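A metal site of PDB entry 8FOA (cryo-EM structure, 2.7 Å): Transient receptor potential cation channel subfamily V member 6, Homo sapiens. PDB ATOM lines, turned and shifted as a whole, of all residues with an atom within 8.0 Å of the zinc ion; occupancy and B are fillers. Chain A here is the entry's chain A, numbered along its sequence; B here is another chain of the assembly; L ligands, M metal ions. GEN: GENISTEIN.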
ATOM      1  N   GLY A 579       5.705  18.615   2.252  1.00  0.00           N
ATOM      2  CA  GLY A 579       4.723  19.222   1.378  1.00  0.00           C
ATOM      3  C   GLY A 579       5.356  20.134   0.350  1.00  0.00           C
ATOM      4  O   GLY A 579       4.788  20.379  -0.718  1.00  0.00           O
ATOM      5  N   HIS A 582       6.916  17.813  -2.491  1.00  0.00           N
ATOM      6  CA  HIS A 582       5.925  17.323  -3.447  1.00  0.00           C
ATOM      7  C   HIS A 582       5.576  18.383  -4.483  1.00  0.00           C
ATOM      8  O   HIS A 582       5.327  18.055  -5.647  1.00  0.00           O
ATOM      9  CB  HIS A 582       4.663  16.871  -2.699  1.00  0.00           C
ATOM     10  CG  HIS A 582       3.527  16.538  -3.612  1.00  0.00           C
ATOM     11  ND1 HIS A 582       3.477  15.371  -4.345  1.00  0.00           N
ATOM     12  CD2 HIS A 582       2.410  17.232  -3.939  1.00  0.00           C
ATOM     13  CE1 HIS A 582       2.371  15.351  -5.064  1.00  0.00           C
ATOM     14  NE2 HIS A 582       1.712  16.477  -4.844  1.00  0.00           N
ATOM     15  N   TRP A 583       5.564  19.644  -4.082  1.00  0.00           N
ATOM     16  CA  TRP A 583       5.150  20.698  -4.995  1.00  0.00           C
ATOM     17  C   TRP A 583       6.212  20.975  -6.055  1.00  0.00           C
ATOM     18  O   TRP A 583       5.891  21.402  -7.169  1.00  0.00           O
ATOM     19  CB  TRP A 583       4.835  21.980  -4.222  1.00  0.00           C
ATOM     20  CG  TRP A 583       4.298  23.072  -5.074  1.00  0.00           C
ATOM     21  CD1 TRP A 583       4.987  24.137  -5.572  1.00  0.00           C
ATOM     22  CD2 TRP A 583       2.958  23.208  -5.554  1.00  0.00           C
ATOM     23  NE1 TRP A 583       4.154  24.928  -6.327  1.00  0.00           N
ATOM     24  CE2 TRP A 583       2.902  24.375  -6.330  1.00  0.00           C
ATOM     25  CE3 TRP A 583       1.787  22.449  -5.392  1.00  0.00           C
ATOM     26  CZ2 TRP A 583       1.731  24.802  -6.946  1.00  0.00           C
ATOM     27  CZ3 TRP A 583       0.633  22.873  -6.007  1.00  0.00           C
ATOM     28  CH2 TRP A 583       0.611  24.043  -6.769  1.00  0.00           C
ATOM     29  N   ALA A 586       6.337  17.260  -8.363  1.00  0.00           N
ATOM     30  CA  ALA A 586       5.139  16.928  -9.120  1.00  0.00           C
ATOM     31  C   ALA A 586       4.483  18.123  -9.801  1.00  0.00           C
ATOM     32  O   ALA A 586       3.795  17.927 -10.811  1.00  0.00           O
ATOM     33  CB  ALA A 586       4.108  16.244  -8.215  1.00  0.00           C
ATOM     34  N   HIS A 587       4.678  19.343  -9.313  1.00  0.00           N
ATOM     35  CA  HIS A 587       3.896  20.449  -9.839  1.00  0.00           C
ATOM     36  C   HIS A 587       4.739  21.530 -10.503  1.00  0.00           C
ATOM     37  O   HIS A 587       4.359  22.048 -11.552  1.00  0.00           O
ATOM     38  CB  HIS A 587       3.037  21.066  -8.732  1.00  0.00           C
ATOM     39  CG  HIS A 587       2.003  20.126  -8.195  1.00  0.00           C
ATOM     40  ND1 HIS A 587       0.844  19.843  -8.885  1.00  0.00           N
ATOM     41  CD2 HIS A 587       1.954  19.415  -7.057  1.00  0.00           C
ATOM     42  CE1 HIS A 587       0.128  18.988  -8.174  1.00  0.00           C
ATOM     43  NE2 HIS A 587       0.774  18.714  -7.058  1.00  0.00           N
ATOM     44  N   TRP B 583      -2.261  18.113   3.242  1.00  0.00           N
ATOM     45  CA  TRP B 583      -2.246  17.858   1.805  1.00  0.00           C
ATOM     46  C   TRP B 583      -2.926  18.983   1.038  1.00  0.00           C
ATOM     47  O   TRP B 583      -2.627  19.231  -0.127  1.00  0.00           O
ATOM     48  CB  TRP B 583      -2.905  16.513   1.528  1.00  0.00           C
ATOM     49  CG  TRP B 583      -2.903  16.102   0.098  1.00  0.00           C
ATOM     50  CD1 TRP B 583      -3.971  16.062  -0.748  1.00  0.00           C
ATOM     51  CD2 TRP B 583      -1.770  15.692  -0.675  1.00  0.00           C
ATOM     52  NE1 TRP B 583      -3.582  15.642  -1.992  1.00  0.00           N
ATOM     53  CE2 TRP B 583      -2.237  15.400  -1.966  1.00  0.00           C
ATOM     54  CE3 TRP B 583      -0.417  15.529  -0.389  1.00  0.00           C
ATOM     55  CZ2 TRP B 583      -1.382  14.965  -2.978  1.00  0.00           C
ATOM     56  CZ3 TRP B 583       0.414  15.102  -1.387  1.00  0.00           C
ATOM     57  CH2 TRP B 583      -0.069  14.822  -2.670  1.00  0.00           C
ATOM     58  N   ALA B 586      -0.535  22.369   1.530  1.00  0.00           N
ATOM     59  CA  ALA B 586       0.635  22.322   0.661  1.00  0.00           C
ATOM     60  C   ALA B 586       0.304  22.695  -0.772  1.00  0.00           C
ATOM     61  O   ALA B 586       1.181  23.147  -1.519  1.00  0.00           O
ATOM     62  CB  ALA B 586       1.265  20.923   0.702  1.00  0.00           C
ATOM     63  N   HIS B 587      -0.953  22.534  -1.176  1.00  0.00           N
ATOM     64  CA  HIS B 587      -1.398  22.883  -2.514  1.00  0.00           C
ATOM     65  C   HIS B 587      -2.059  24.261  -2.582  1.00  0.00           C
ATOM     66  O   HIS B 587      -2.292  24.752  -3.684  1.00  0.00           O
ATOM     67  CB  HIS B 587      -2.373  21.827  -3.040  1.00  0.00           C
ATOM     68  CG  HIS B 587      -1.740  20.497  -3.277  1.00  0.00           C
ATOM     69  ND1 HIS B 587      -1.637  19.545  -2.297  1.00  0.00           N
ATOM     70  CD2 HIS B 587      -1.197  19.952  -4.395  1.00  0.00           C
ATOM     71  CE1 HIS B 587      -1.042  18.473  -2.787  1.00  0.00           C
ATOM     72  NE2 HIS B 587      -0.769  18.690  -4.064  1.00  0.00           N
HETATM   73  C1  GEN L   1       5.024   9.042   1.287  1.00  0.00           C
HETATM   74  C2  GEN L   1       4.431   7.895   1.661  1.00  0.00           C
HETATM   75  O2  GEN L   1       5.044   6.647   1.373  1.00  0.00           O
HETATM   76  C3  GEN L   1       3.197   7.913   2.323  1.00  0.00           C
HETATM   77  C4  GEN L   1       2.594   9.112   2.598  1.00  0.00           C
HETATM   78  O4  GEN L   1       1.411   9.138   3.240  1.00  0.00           O
HETATM   79  C5  GEN L   1       3.231  10.330   2.215  1.00  0.00           C
HETATM   80  C6  GEN L   1       2.632  11.578   2.484  1.00  0.00           C
HETATM   81  O6  GEN L   1       1.419  11.642   3.141  1.00  0.00           O
HETATM   82  C7  GEN L   1       3.380  12.788   2.033  1.00  0.00           C
HETATM   83  C8  GEN L   1       4.545  12.613   1.400  1.00  0.00           C
HETATM   84  O9  GEN L   1       5.038  11.458   1.190  1.00  0.00           O
HETATM   85  C10 GEN L   1       4.407  10.299   1.578  1.00  0.00           C
HETATM   86  C11 GEN L   1       2.864  14.212   2.273  1.00  0.00           C
HETATM   87  C12 GEN L   1       2.417  14.579   3.521  1.00  0.00           C
HETATM   88  C13 GEN L   1       1.947  15.876   3.766  1.00  0.00           C
HETATM   89  C14 GEN L   1       1.956  16.777   2.756  1.00  0.00           C
HETATM   90  O14 GEN L   1       1.486  18.106   3.010  1.00  0.00           O
HETATM   91  C15 GEN L   1       2.431  16.411   1.468  1.00  0.00           C
HETATM   92  C16 GEN L   1       2.878  15.157   1.234  1.00  0.00           C
HETATM   93 ZN    ZN M   1      -0.197  17.221  -5.758  1.00  0.00          ZN
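ND1 of His 587 of chain B lies within hydrogen-bond range of O of Trp 583 of chain B.
Merely in contact with the zinc ion: Trp 583 of chain B (3.8 Å). Four residues have an atom within 4 Å of the zinc ion: His 582, His 587 of chain A, Trp 583 of chain B and His 587 of chain B. Along chain A the residues within 4 Å of the zinc ion span positions 582 to 587.
The zinc ion is bound by a ring nitrogen (NE2) of His 587 of chain A (2.2 Å), a ring nitrogen (NE2) of His 582 (2.2 Å) and a ring nitrogen (NE2) of His 587 of chain B (2.3 Å). The zinc ion has three donor atoms within binding distance.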
